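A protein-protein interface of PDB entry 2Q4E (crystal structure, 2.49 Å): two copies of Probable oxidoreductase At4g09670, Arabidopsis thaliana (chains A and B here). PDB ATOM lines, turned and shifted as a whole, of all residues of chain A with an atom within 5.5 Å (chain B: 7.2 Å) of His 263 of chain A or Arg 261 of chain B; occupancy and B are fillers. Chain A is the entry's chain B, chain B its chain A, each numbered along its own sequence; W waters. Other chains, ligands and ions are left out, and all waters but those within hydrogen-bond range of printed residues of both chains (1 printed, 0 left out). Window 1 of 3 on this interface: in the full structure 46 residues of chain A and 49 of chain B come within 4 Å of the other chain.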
ATOM      1  N   THR A 248      -7.590  20.897  12.718  1.00  0.00           N
ATOM      2  CA  THR A 248      -7.107  20.466  14.031  1.00  0.00           C
ATOM      3  C   THR A 248      -5.729  19.840  13.859  1.00  0.00           C
ATOM      4  O   THR A 248      -5.563  18.911  13.079  1.00  0.00           O
ATOM      5  CB  THR A 248      -8.009  19.381  14.678  1.00  0.00           C
ATOM      6  OG1 THR A 248      -9.371  19.824  14.725  1.00  0.00           O
ATOM      7  CG2 THR A 248      -7.531  19.090  16.101  1.00  0.00           C
ATOM      8  N   MET A 249      -4.752  20.343  14.604  1.00  0.00           N
ATOM      9  CA  MET A 249      -3.385  19.838  14.532  1.00  0.00           C
ATOM     10  C   MET A 249      -2.821  19.828  15.941  1.00  0.00           C
ATOM     11  O   MET A 249      -3.241  20.629  16.781  1.00  0.00           O
ATOM     12  CB  MET A 249      -2.532  20.747  13.648  1.00  0.00           C
ATOM     13  CG  MET A 249      -2.358  22.129  14.224  1.00  0.00           C
ATOM     14  SD  MET A 249      -1.695  23.441  12.980  1.00  0.00           S
ATOM     15  CE  MET A 249      -3.210  23.439  11.788  1.00  0.00           C
ATOM     16  N   GLU A 250      -1.869  18.934  16.194  1.00  0.00           N
ATOM     17  CA  GLU A 250      -1.264  18.827  17.516  1.00  0.00           C
ATOM     18  C   GLU A 250      -0.331  17.627  17.654  1.00  0.00           C
ATOM     19  O   GLU A 250      -0.352  16.689  16.846  1.00  0.00           O
ATOM     20  CB  GLU A 250      -2.344  18.667  18.585  1.00  0.00           C
ATOM     21  CG  GLU A 250      -3.014  17.289  18.544  1.00  0.00           C
ATOM     22  CD  GLU A 250      -3.812  16.971  19.794  1.00  0.00           C
ATOM     23  OE1 GLU A 250      -3.238  17.043  20.902  1.00  0.00           O
ATOM     24  OE2 GLU A 250      -5.012  16.642  19.669  1.00  0.00           O
ATOM     25  N   ILE A 251       0.481  17.679  18.701  1.00  0.00           N
ATOM     26  CA  ILE A 251       1.385  16.597  19.037  1.00  0.00           C
ATOM     27  C   ILE A 251       1.102  16.318  20.504  1.00  0.00           C
ATOM     28  O   ILE A 251       1.010  17.247  21.304  1.00  0.00           O
ATOM     29  CB  ILE A 251       2.872  16.975  18.971  1.00  0.00           C
ATOM     30  CG1 ILE A 251       3.223  17.614  17.634  1.00  0.00           C
ATOM     31  CG2 ILE A 251       3.701  15.720  19.211  1.00  0.00           C
ATOM     32  CD1 ILE A 251       4.661  18.118  17.562  1.00  0.00           C
ATOM     33  N   THR A 252       0.965  15.044  20.853  1.00  0.00           N
ATOM     34  CA  THR A 252       0.734  14.652  22.235  1.00  0.00           C
ATOM     35  C   THR A 252       1.664  13.504  22.602  1.00  0.00           C
ATOM     36  O   THR A 252       1.341  12.336  22.385  1.00  0.00           O
ATOM     37  CB  THR A 252      -0.713  14.211  22.476  1.00  0.00           C
ATOM     38  OG1 THR A 252      -1.579  15.339  22.322  1.00  0.00           O
ATOM     39  CG2 THR A 252      -0.877  13.677  23.884  1.00  0.00           C
ATOM     40  N   ARG A 261       2.690  18.757  24.859  1.00  0.00           N
ATOM     41  CA  ARG A 261       1.500  19.130  24.114  1.00  0.00           C
ATOM     42  C   ARG A 261       1.629  20.442  23.347  1.00  0.00           C
ATOM     43  O   ARG A 261       2.010  21.484  23.899  1.00  0.00           O
ATOM     44  CB  ARG A 261       0.287  19.211  25.053  1.00  0.00           C
ATOM     45  CG  ARG A 261      -0.810  18.188  24.762  1.00  0.00           C
ATOM     46  CD  ARG A 261      -1.544  17.783  26.041  1.00  0.00           C
ATOM     47  NE  ARG A 261      -2.167  18.919  26.717  1.00  0.00           N
ATOM     48  CZ  ARG A 261      -2.457  18.953  28.013  1.00  0.00           C
ATOM     49  NH1 ARG A 261      -2.181  17.908  28.793  1.00  0.00           N
ATOM     50  NH2 ARG A 261      -3.015  20.034  28.536  1.00  0.00           N
ATOM     51  N   VAL A 262       1.309  20.365  22.063  1.00  0.00           N
ATOM     52  CA  VAL A 262       1.322  21.516  21.183  1.00  0.00           C
ATOM     53  C   VAL A 262       0.195  21.299  20.184  1.00  0.00           C
ATOM     54  O   VAL A 262       0.117  20.250  19.560  1.00  0.00           O
ATOM     55  CB  VAL A 262       2.693  21.684  20.469  1.00  0.00           C
ATOM     56  CG1 VAL A 262       3.275  20.346  20.113  1.00  0.00           C
ATOM     57  CG2 VAL A 262       2.523  22.558  19.234  1.00  0.00           C
ATOM     58  N   HIS A 263      -0.686  22.287  20.060  1.00  0.00           N
ATOM     59  CA  HIS A 263      -1.845  22.206  19.173  1.00  0.00           C
ATOM     60  C   HIS A 263      -1.747  23.053  17.906  1.00  0.00           C
ATOM     61  O   HIS A 263      -2.753  23.297  17.234  1.00  0.00           O
ATOM     62  CB  HIS A 263      -3.101  22.617  19.942  1.00  0.00           C
ATOM     63  CG  HIS A 263      -3.271  21.907  21.248  1.00  0.00           C
ATOM     64  ND1 HIS A 263      -3.455  20.544  21.337  1.00  0.00           N
ATOM     65  CD2 HIS A 263      -3.291  22.372  22.520  1.00  0.00           C
ATOM     66  CE1 HIS A 263      -3.581  20.201  22.606  1.00  0.00           C
ATOM     67  NE2 HIS A 263      -3.486  21.292  23.346  1.00  0.00           N
ATOM     68  N   ASP A 264      -0.540  23.504  17.586  1.00  0.00           N
ATOM     69  CA  ASP A 264      -0.320  24.322  16.399  1.00  0.00           C
ATOM     70  C   ASP A 264       1.099  24.063  15.913  1.00  0.00           C
ATOM     71  O   ASP A 264       1.800  24.987  15.485  1.00  0.00           O
ATOM     72  CB  ASP A 264      -0.498  25.804  16.752  1.00  0.00           C
ATOM     73  CG  ASP A 264       0.512  26.280  17.773  1.00  0.00           C
ATOM     74  OD1 ASP A 264       1.166  25.411  18.380  1.00  0.00           O
ATOM     75  OD2 ASP A 264       0.646  27.512  17.974  1.00  0.00           O
ATOM     76  N   PHE A 265       1.508  22.795  15.958  1.00  0.00           N
ATOM     77  CA  PHE A 265       2.866  22.413  15.573  1.00  0.00           C
ATOM     78  C   PHE A 265       3.187  22.512  14.082  1.00  0.00           C
ATOM     79  O   PHE A 265       4.359  22.559  13.710  1.00  0.00           O
ATOM     80  CB  PHE A 265       3.192  21.001  16.114  1.00  0.00           C
ATOM     81  CG  PHE A 265       2.864  19.877  15.164  1.00  0.00           C
ATOM     82  CD1 PHE A 265       3.808  19.428  14.232  1.00  0.00           C
ATOM     83  CD2 PHE A 265       1.619  19.249  15.209  1.00  0.00           C
ATOM     84  CE1 PHE A 265       3.510  18.364  13.362  1.00  0.00           C
ATOM     85  CE2 PHE A 265       1.317  18.195  14.349  1.00  0.00           C
ATOM     86  CZ  PHE A 265       2.265  17.751  13.426  1.00  0.00           C
ATOM     87  N   TYR A 269      -0.163  29.624  15.587  1.00  0.00           N
ATOM     88  CA  TYR A 269      -1.268  30.579  15.626  1.00  0.00           C
ATOM     89  C   TYR A 269      -0.754  31.904  15.069  1.00  0.00           C
ATOM     90  O   TYR A 269      -1.342  32.479  14.148  1.00  0.00           O
ATOM     91  CB  TYR A 269      -1.773  30.764  17.064  1.00  0.00           C
ATOM     92  CG  TYR A 269      -2.542  29.574  17.616  1.00  0.00           C
ATOM     93  CD1 TYR A 269      -3.455  28.877  16.821  1.00  0.00           C
ATOM     94  CD2 TYR A 269      -2.370  29.155  18.939  1.00  0.00           C
ATOM     95  CE1 TYR A 269      -4.172  27.800  17.318  1.00  0.00           C
ATOM     96  CE2 TYR A 269      -3.087  28.071  19.449  1.00  0.00           C
ATOM     97  CZ  TYR A 269      -3.987  27.401  18.629  1.00  0.00           C
ATOM     98  OH  TYR A 269      -4.708  26.328  19.111  1.00  0.00           O
ATOM     99  N   SER A 275       4.076  28.376  21.232  1.00  0.00           N
ATOM    100  CA  SER A 275       3.904  27.832  22.571  1.00  0.00           C
ATOM    101  C   SER A 275       3.756  26.312  22.608  1.00  0.00           C
ATOM    102  O   SER A 275       3.250  25.695  21.667  1.00  0.00           O
ATOM    103  CB  SER A 275       2.692  28.477  23.245  1.00  0.00           C
ATOM    104  OG  SER A 275       2.829  29.881  23.271  1.00  0.00           O
ATOM    105  N   LEU B 140     -21.385  20.374  26.655  1.00  0.00           N
ATOM    106  CA  LEU B 140     -20.288  19.807  25.883  1.00  0.00           C
ATOM    107  C   LEU B 140     -20.858  18.571  25.205  1.00  0.00           C
ATOM    108  O   LEU B 140     -20.510  18.244  24.070  1.00  0.00           O
ATOM    109  CB  LEU B 140     -19.137  19.436  26.814  1.00  0.00           C
ATOM    110  CG  LEU B 140     -18.012  18.560  26.278  1.00  0.00           C
ATOM    111  CD1 LEU B 140     -16.752  18.801  27.096  1.00  0.00           C
ATOM    112  CD2 LEU B 140     -18.448  17.104  26.330  1.00  0.00           C
ATOM    113  N   PHE B 143     -22.461  20.589  23.161  1.00  0.00           N
ATOM    114  CA  PHE B 143     -21.550  21.293  22.262  1.00  0.00           C
ATOM    115  C   PHE B 143     -21.235  20.425  21.055  1.00  0.00           C
ATOM    116  O   PHE B 143     -20.859  20.929  20.001  1.00  0.00           O
ATOM    117  CB  PHE B 143     -20.238  21.643  22.965  1.00  0.00           C
ATOM    118  CG  PHE B 143     -19.211  22.249  22.049  1.00  0.00           C
ATOM    119  CD1 PHE B 143     -19.269  23.595  21.714  1.00  0.00           C
ATOM    120  CD2 PHE B 143     -18.219  21.457  21.478  1.00  0.00           C
ATOM    121  CE1 PHE B 143     -18.358  24.152  20.818  1.00  0.00           C
ATOM    122  CE2 PHE B 143     -17.302  22.002  20.581  1.00  0.00           C
ATOM    123  CZ  PHE B 143     -17.373  23.353  20.249  1.00  0.00           C
ATOM    124  N   LEU B 144     -21.386  19.115  21.222  1.00  0.00           N
ATOM    125  CA  LEU B 144     -21.115  18.167  20.154  1.00  0.00           C
ATOM    126  C   LEU B 144     -22.407  17.750  19.464  1.00  0.00           C
ATOM    127  O   LEU B 144     -22.390  16.934  18.550  1.00  0.00           O
ATOM    128  CB  LEU B 144     -20.397  16.936  20.716  1.00  0.00           C
ATOM    129  CG  LEU B 144     -19.143  17.234  21.553  1.00  0.00           C
ATOM    130  CD1 LEU B 144     -18.492  15.928  21.988  1.00  0.00           C
ATOM    131  CD2 LEU B 144     -18.163  18.074  20.744  1.00  0.00           C
ATOM    132  N   GLU B 250      -6.878  13.056  27.991  1.00  0.00           N
ATOM    133  CA  GLU B 250      -7.386  13.806  26.854  1.00  0.00           C
ATOM    134  C   GLU B 250      -8.521  13.144  26.100  1.00  0.00           C
ATOM    135  O   GLU B 250      -8.652  11.921  26.069  1.00  0.00           O
ATOM    136  CB  GLU B 250      -6.253  14.097  25.864  1.00  0.00           C
ATOM    137  CG  GLU B 250      -5.691  15.508  25.940  1.00  0.00           C
ATOM    138  CD  GLU B 250      -6.147  16.400  24.785  1.00  0.00           C
ATOM    139  OE1 GLU B 250      -7.349  16.742  24.709  1.00  0.00           O
ATOM    140  OE2 GLU B 250      -5.291  16.756  23.946  1.00  0.00           O
ATOM    141  N   ILE B 251      -9.354  13.990  25.510  1.00  0.00           N
ATOM    142  CA  ILE B 251     -10.462  13.547  24.679  1.00  0.00           C
ATOM    143  C   ILE B 251     -10.290  14.350  23.402  1.00  0.00           C
ATOM    144  O   ILE B 251     -10.283  15.578  23.451  1.00  0.00           O
ATOM    145  CB  ILE B 251     -11.844  13.928  25.252  1.00  0.00           C
ATOM    146  CG1 ILE B 251     -12.190  13.059  26.460  1.00  0.00           C
ATOM    147  CG2 ILE B 251     -12.905  13.780  24.169  1.00  0.00           C
ATOM    148  CD1 ILE B 251     -13.498  13.462  27.137  1.00  0.00           C
ATOM    149  N   THR B 252     -10.101  13.681  22.272  1.00  0.00           N
ATOM    150  CA  THR B 252     -10.014  14.410  21.007  1.00  0.00           C
ATOM    151  C   THR B 252     -11.239  14.032  20.189  1.00  0.00           C
ATOM    152  O   THR B 252     -11.482  12.854  19.929  1.00  0.00           O
ATOM    153  CB  THR B 252      -8.753  14.070  20.195  1.00  0.00           C
ATOM    154  OG1 THR B 252      -7.602  14.612  20.845  1.00  0.00           O
ATOM    155  CG2 THR B 252      -8.849  14.670  18.796  1.00  0.00           C
ATOM    156  N   ALA B 253     -12.027  15.034  19.814  1.00  0.00           N
ATOM    157  CA  ALA B 253     -13.228  14.810  19.013  1.00  0.00           C
ATOM    158  C   ALA B 253     -13.143  15.686  17.777  1.00  0.00           C
ATOM    159  O   ALA B 253     -13.082  16.909  17.879  1.00  0.00           O
ATOM    160  CB  ALA B 253     -14.481  15.153  19.828  1.00  0.00           C
ATOM    161  N   THR B 259     -14.261  21.169  16.546  1.00  0.00           N
ATOM    162  CA  THR B 259     -13.246  20.342  17.178  1.00  0.00           C
ATOM    163  C   THR B 259     -13.358  20.535  18.685  1.00  0.00           C
ATOM    164  O   THR B 259     -13.348  21.664  19.173  1.00  0.00           O
ATOM    165  CB  THR B 259     -11.839  20.758  16.713  1.00  0.00           C
ATOM    166  OG1 THR B 259     -11.740  20.573  15.300  1.00  0.00           O
ATOM    167  CG2 THR B 259     -10.761  19.928  17.406  1.00  0.00           C
ATOM    168  N   LEU B 260     -13.482  19.434  19.418  1.00  0.00           N
ATOM    169  CA  LEU B 260     -13.591  19.507  20.865  1.00  0.00           C
ATOM    170  C   LEU B 260     -12.394  18.841  21.527  1.00  0.00           C
ATOM    171  O   LEU B 260     -11.962  17.766  21.105  1.00  0.00           O
ATOM    172  CB  LEU B 260     -14.862  18.810  21.336  1.00  0.00           C
ATOM    173  CG  LEU B 260     -14.935  18.740  22.861  1.00  0.00           C
ATOM    174  CD1 LEU B 260     -15.403  20.083  23.389  1.00  0.00           C
ATOM    175  CD2 LEU B 260     -15.873  17.631  23.302  1.00  0.00           C
ATOM    176  N   ARG B 261     -11.863  19.476  22.570  1.00  0.00           N
ATOM    177  CA  ARG B 261     -10.720  18.920  23.281  1.00  0.00           C
ATOM    178  C   ARG B 261     -10.851  19.082  24.791  1.00  0.00           C
ATOM    179  O   ARG B 261     -11.314  20.116  25.281  1.00  0.00           O
ATOM    180  CB  ARG B 261      -9.410  19.579  22.814  1.00  0.00           C
ATOM    181  CG  ARG B 261      -9.067  19.351  21.342  1.00  0.00           C
ATOM    182  CD  ARG B 261      -7.568  19.492  21.083  1.00  0.00           C
ATOM    183  NE  ARG B 261      -7.063  20.819  21.431  1.00  0.00           N
ATOM    184  CZ  ARG B 261      -7.144  21.897  20.650  1.00  0.00           C
ATOM    185  NH1 ARG B 261      -7.709  21.822  19.446  1.00  0.00           N
ATOM    186  NH2 ARG B 261      -6.662  23.058  21.082  1.00  0.00           N
ATOM    187  N   VAL B 262     -10.441  18.053  25.528  1.00  0.00           N
ATOM    188  CA  VAL B 262     -10.485  18.104  26.981  1.00  0.00           C
ATOM    189  C   VAL B 262      -9.144  17.614  27.530  1.00  0.00           C
ATOM    190  O   VAL B 262      -8.771  16.454  27.350  1.00  0.00           O
ATOM    191  CB  VAL B 262     -11.629  17.230  27.543  1.00  0.00           C
ATOM    192  CG1 VAL B 262     -11.933  17.632  28.985  1.00  0.00           C
ATOM    193  CG2 VAL B 262     -12.871  17.381  26.681  1.00  0.00           C
ATOM    194  N   HIS B 263      -8.420  18.508  28.195  1.00  0.00           N
ATOM    195  CA  HIS B 263      -7.116  18.171  28.758  1.00  0.00           C
ATOM    196  C   HIS B 263      -7.232  17.409  30.070  1.00  0.00           C
ATOM    197  O   HIS B 263      -6.259  16.825  30.559  1.00  0.00           O
ATOM    198  CB  HIS B 263      -6.297  19.441  28.939  1.00  0.00           C
ATOM    199  CG  HIS B 263      -6.146  20.231  27.676  1.00  0.00           C
ATOM    200  ND1 HIS B 263      -5.574  19.708  26.535  1.00  0.00           N
ATOM    201  CD2 HIS B 263      -6.515  21.498  27.365  1.00  0.00           C
ATOM    202  CE1 HIS B 263      -5.599  20.616  25.579  1.00  0.00           C
ATOM    203  NE2 HIS B 263      -6.164  21.710  26.056  1.00  0.00           N
ATOM    204  N   ASP B 264      -8.426  17.437  30.646  1.00  0.00           N
ATOM    205  CA  ASP B 264      -8.702  16.698  31.868  1.00  0.00           C
ATOM    206  C   ASP B 264      -9.834  15.734  31.525  1.00  0.00           C
ATOM    207  O   ASP B 264      -9.643  14.813  30.739  1.00  0.00           O
ATOM    208  CB  ASP B 264      -9.115  17.637  33.002  1.00  0.00           C
ATOM    209  CG  ASP B 264      -9.870  18.864  32.513  1.00  0.00           C
ATOM    210  OD1 ASP B 264     -10.726  18.740  31.612  1.00  0.00           O
ATOM    211  OD2 ASP B 264      -9.610  19.954  33.051  1.00  0.00           O
ATOM    212  N   SER B 275     -13.120  23.005  32.580  1.00  0.00           N
ATOM    213  CA  SER B 275     -12.988  23.622  31.264  1.00  0.00           C
ATOM    214  C   SER B 275     -12.692  22.662  30.110  1.00  0.00           C
ATOM    215  O   SER B 275     -12.250  21.538  30.325  1.00  0.00           O
ATOM    216  CB  SER B 275     -11.898  24.695  31.316  1.00  0.00           C
ATOM    217  OG  SER B 275     -12.224  25.696  32.258  1.00  0.00           O
ATOM    218  N   PHE B 276     -12.940  23.125  28.887  1.00  0.00           N
ATOM    219  CA  PHE B 276     -12.684  22.342  27.681  1.00  0.00           C
ATOM    220  C   PHE B 276     -12.480  23.269  26.481  1.00  0.00           C
ATOM    221  O   PHE B 276     -12.865  24.441  26.523  1.00  0.00           O
ATOM    222  CB  PHE B 276     -13.832  21.355  27.423  1.00  0.00           C
ATOM    223  CG  PHE B 276     -15.187  22.002  27.292  1.00  0.00           C
ATOM    224  CD1 PHE B 276     -15.583  22.588  26.093  1.00  0.00           C
ATOM    225  CD2 PHE B 276     -16.067  22.022  28.371  1.00  0.00           C
ATOM    226  CE1 PHE B 276     -16.835  23.180  25.970  1.00  0.00           C
ATOM    227  CE2 PHE B 276     -17.318  22.611  28.256  1.00  0.00           C
ATOM    228  CZ  PHE B 276     -17.703  23.194  27.050  1.00  0.00           C
ATOM    229  N   THR B 277     -11.860  22.752  25.423  1.00  0.00           N
ATOM    230  CA  THR B 277     -11.585  23.541  24.222  1.00  0.00           C
ATOM    231  C   THR B 277     -12.833  23.691  23.361  1.00  0.00           C
ATOM    232  O   THR B 277     -13.845  23.055  23.625  1.00  0.00           O
ATOM    233  CB  THR B 277     -10.479  22.886  23.368  1.00  0.00           C
ATOM    234  OG1 THR B 277      -9.332  22.636  24.190  1.00  0.00           O
ATOM    235  CG2 THR B 277     -10.073  23.798  22.214  1.00  0.00           C
ATOM    236  N   THR B 278     -12.748  24.530  22.330  1.00  0.00           N
ATOM    237  CA  THR B 278     -13.868  24.781  21.426  1.00  0.00           C
ATOM    238  C   THR B 278     -13.378  25.436  20.133  1.00  0.00           C
ATOM    239  O   THR B 278     -12.684  26.448  20.178  1.00  0.00           O
ATOM    240  CB  THR B 278     -14.903  25.715  22.099  1.00  0.00           C
ATOM    241  OG1 THR B 278     -15.661  24.972  23.059  1.00  0.00           O
ATOM    242  CG2 THR B 278     -15.832  26.335  21.074  1.00  0.00           C
ATOM    243  N   SER B 279     -13.744  24.868  18.987  1.00  0.00           N
ATOM    244  CA  SER B 279     -13.327  25.421  17.695  1.00  0.00           C
ATOM    245  C   SER B 279     -14.291  25.104  16.556  1.00  0.00           C
ATOM    246  O   SER B 279     -14.698  23.955  16.369  1.00  0.00           O
ATOM    247  CB  SER B 279     -11.934  24.909  17.312  1.00  0.00           C
ATOM    248  OG  SER B 279     -11.671  25.150  15.938  1.00  0.00           O
ATOM    249  N   TRP B 291      -3.585  31.527  11.864  1.00  0.00           N
ATOM    250  CA  TRP B 291      -4.966  31.090  12.106  1.00  0.00           C
ATOM    251  C   TRP B 291      -5.851  32.330  12.154  1.00  0.00           C
ATOM    252  O   TRP B 291      -5.529  33.294  12.851  1.00  0.00           O
ATOM    253  CB  TRP B 291      -5.086  30.358  13.450  1.00  0.00           C
ATOM    254  CG  TRP B 291      -4.479  28.992  13.491  1.00  0.00           C
ATOM    255  CD1 TRP B 291      -3.175  28.660  13.246  1.00  0.00           C
ATOM    256  CD2 TRP B 291      -5.142  27.773  13.849  1.00  0.00           C
ATOM    257  NE1 TRP B 291      -2.986  27.313  13.436  1.00  0.00           N
ATOM    258  CE2 TRP B 291      -4.176  26.744  13.807  1.00  0.00           C
ATOM    259  CE3 TRP B 291      -6.461  27.450  14.206  1.00  0.00           C
ATOM    260  CZ2 TRP B 291      -4.486  25.411  14.107  1.00  0.00           C
ATOM    261  CZ3 TRP B 291      -6.769  26.124  14.505  1.00  0.00           C
ATOM    262  CH2 TRP B 291      -5.784  25.122  14.455  1.00  0.00           C
ATOM    263  N   PRO B 295      -9.265  28.302  18.253  1.00  0.00           N
ATOM    264  CA  PRO B 295     -10.209  27.705  19.201  1.00  0.00           C
ATOM    265  C   PRO B 295     -10.293  28.404  20.558  1.00  0.00           C
ATOM    266  O   PRO B 295      -9.288  28.863  21.109  1.00  0.00           O
ATOM    267  CB  PRO B 295      -9.721  26.260  19.309  1.00  0.00           C
ATOM    268  CG  PRO B 295      -8.256  26.367  19.035  1.00  0.00           C
ATOM    269  CD  PRO B 295      -8.227  27.327  17.874  1.00  0.00           C
ATOM    270  N   GLU B 297     -11.694  28.509  24.710  1.00  0.00           N
ATOM    271  CA  GLU B 297     -11.865  27.641  25.873  1.00  0.00           C
ATOM    272  C   GLU B 297     -13.033  28.106  26.743  1.00  0.00           C
ATOM    273  O   GLU B 297     -12.988  29.198  27.311  1.00  0.00           O
ATOM    274  CB  GLU B 297     -10.589  27.631  26.718  1.00  0.00           C
ATOM    275  CG  GLU B 297      -9.312  27.394  25.928  1.00  0.00           C
ATOM    276  CD  GLU B 297      -9.423  26.223  24.979  1.00  0.00           C
ATOM    277  OE1 GLU B 297      -9.534  26.452  23.758  1.00  0.00           O
ATOM    278  OE2 GLU B 297      -9.411  25.071  25.453  1.00  0.00           O
HETATM  279  O   HOH W   1      -3.949  15.712  30.135  1.00  0.00           O
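The side-chain hydroxyl (OG1) of Thr 252 of chain B is in hydrogen-bond range of the side-chain carboxylate (OE2) of Glu 250 of chain A.
The backbone NH (N) of Trp 291 of chain B sits at hydrogen-bond distance from the backbone carbonyl oxygen (O) of Tyr 269 of chain A, at 3.3 Å.
The guanidinium group of Arg 261 of chain A lies close to a ring nitrogen (ND1) of His 263 of chain B (3.3 Å).
The side-chain hydroxyl (OG1) of Thr 259 of chain B is in hydrogen-bond range of the side-chain hydroxyl (OG1) of Thr 248 of chain A, 2.6 Å away.
The side-chain carboxylate (OE1) of Glu 250 of chain A is in hydrogen-bond range of the side-chain hydroxyl (OG1) of Thr 252 of chain A, 2.8 Å away.
The side-chain carboxylate (OD2) of Asp 264 of chain A sits at hydrogen-bond distance from the backbone NH (N) of Tyr 269 of chain A.
OE1 of Glu 250 of chain B lies close to N of Val 262 of chain B (3.5 Å).
The backbone NH (N) of Thr 259 of chain B is in hydrogen-bond range of the backbone carbonyl oxygen (O) of Ser 279 of chain B.
N of Thr 277 of chain B sits at hydrogen-bond distance from O of Arg 261 of chain B, 2.7 Å away.
Met 249 of chain A touches Trp 291 of chain B (CE to CZ2, 3.3 Å).
OE1 of Glu 250 of chain A touches OE2 of Glu 250 of chain B, at 3.7 Å.
His 263 of chain A touches Arg 261 of chain B (CG to NH2, 3.6 Å).
His 263 of chain B touches His 263 of chain A.
Tyr 269 of chain A touches Pro 295 of chain B (OH to CG, 3.5 Å).
Of chain B, only Arg 261 (3.6 Å) and His 263 (3.1 Å) come within 4 Å of His 263 of chain A.
Of chain A, only His 263 (3.6 Å) comes within 4 Å of Arg 261 of chain B.
Printed residues of chain A within 4 Å of His 263 of chain B: Arg 261 (3.3 Å) and His 263 (3.1 Å).
Of the printed residues of chain A, Pro 295 of chain B touches Tyr 269.
Of the printed residues of chain A, Trp 291 of chain B touches Met 249 (3.3 Å) and Tyr 269 (3.3 Å).
Of the printed residues of chain B, Tyr 269 of chain A touches Trp 291 and Pro 295.
Printed residues of chain B within 4 Å of Glu 250 of chain A: Glu 250 (3.7 Å) and Thr 252 (3.5 Å).
The nearest residue of chain B that does not touch His 263 of chain A is Glu 250 of chain B (4.1 Å).
The nearest residue of chain A that does not touch Arg 261 of chain B is Glu 250 of chain A (4.1 Å).
The nearest printed residue of chain B that does not touch Tyr 269 of chain A is Arg 261 of chain B (4.3 Å).
Of the 12 printed residues of chain A, 6 touch a printed residue of chain B.
Hydrophobic or aromatic side chains of chain A that line the printed part of chain B: Met 249, His 263 and Tyr 269.
Glu 250 of chain B touches its own counterpart, Glu 250 of chain A.
Glu 250 of chain A touches Thr 252 of chain B, but with the chains exchanged Thr 252 of chain A does not touch Glu 250 of chain B (4.3 Å).
Arg 261 of chain A touches His 263 of chain B, and with the chains exchanged His 263 of chain A touches Arg 261 of chain B.
His 263 of chain B touches its own counterpart, His 263 of chain A.
Positions printed for both chains: 250, 251, 252, 261, 262, 263, 264 and 275.
Of the 9 pairs that touch across the chains among the printed residues, 4 have their exchanged pair printed and touching as well.
Water W1 bridges the backbone carbonyl oxygen of His 263 of chain B and the guanidinium group of Arg 261 of chain A.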
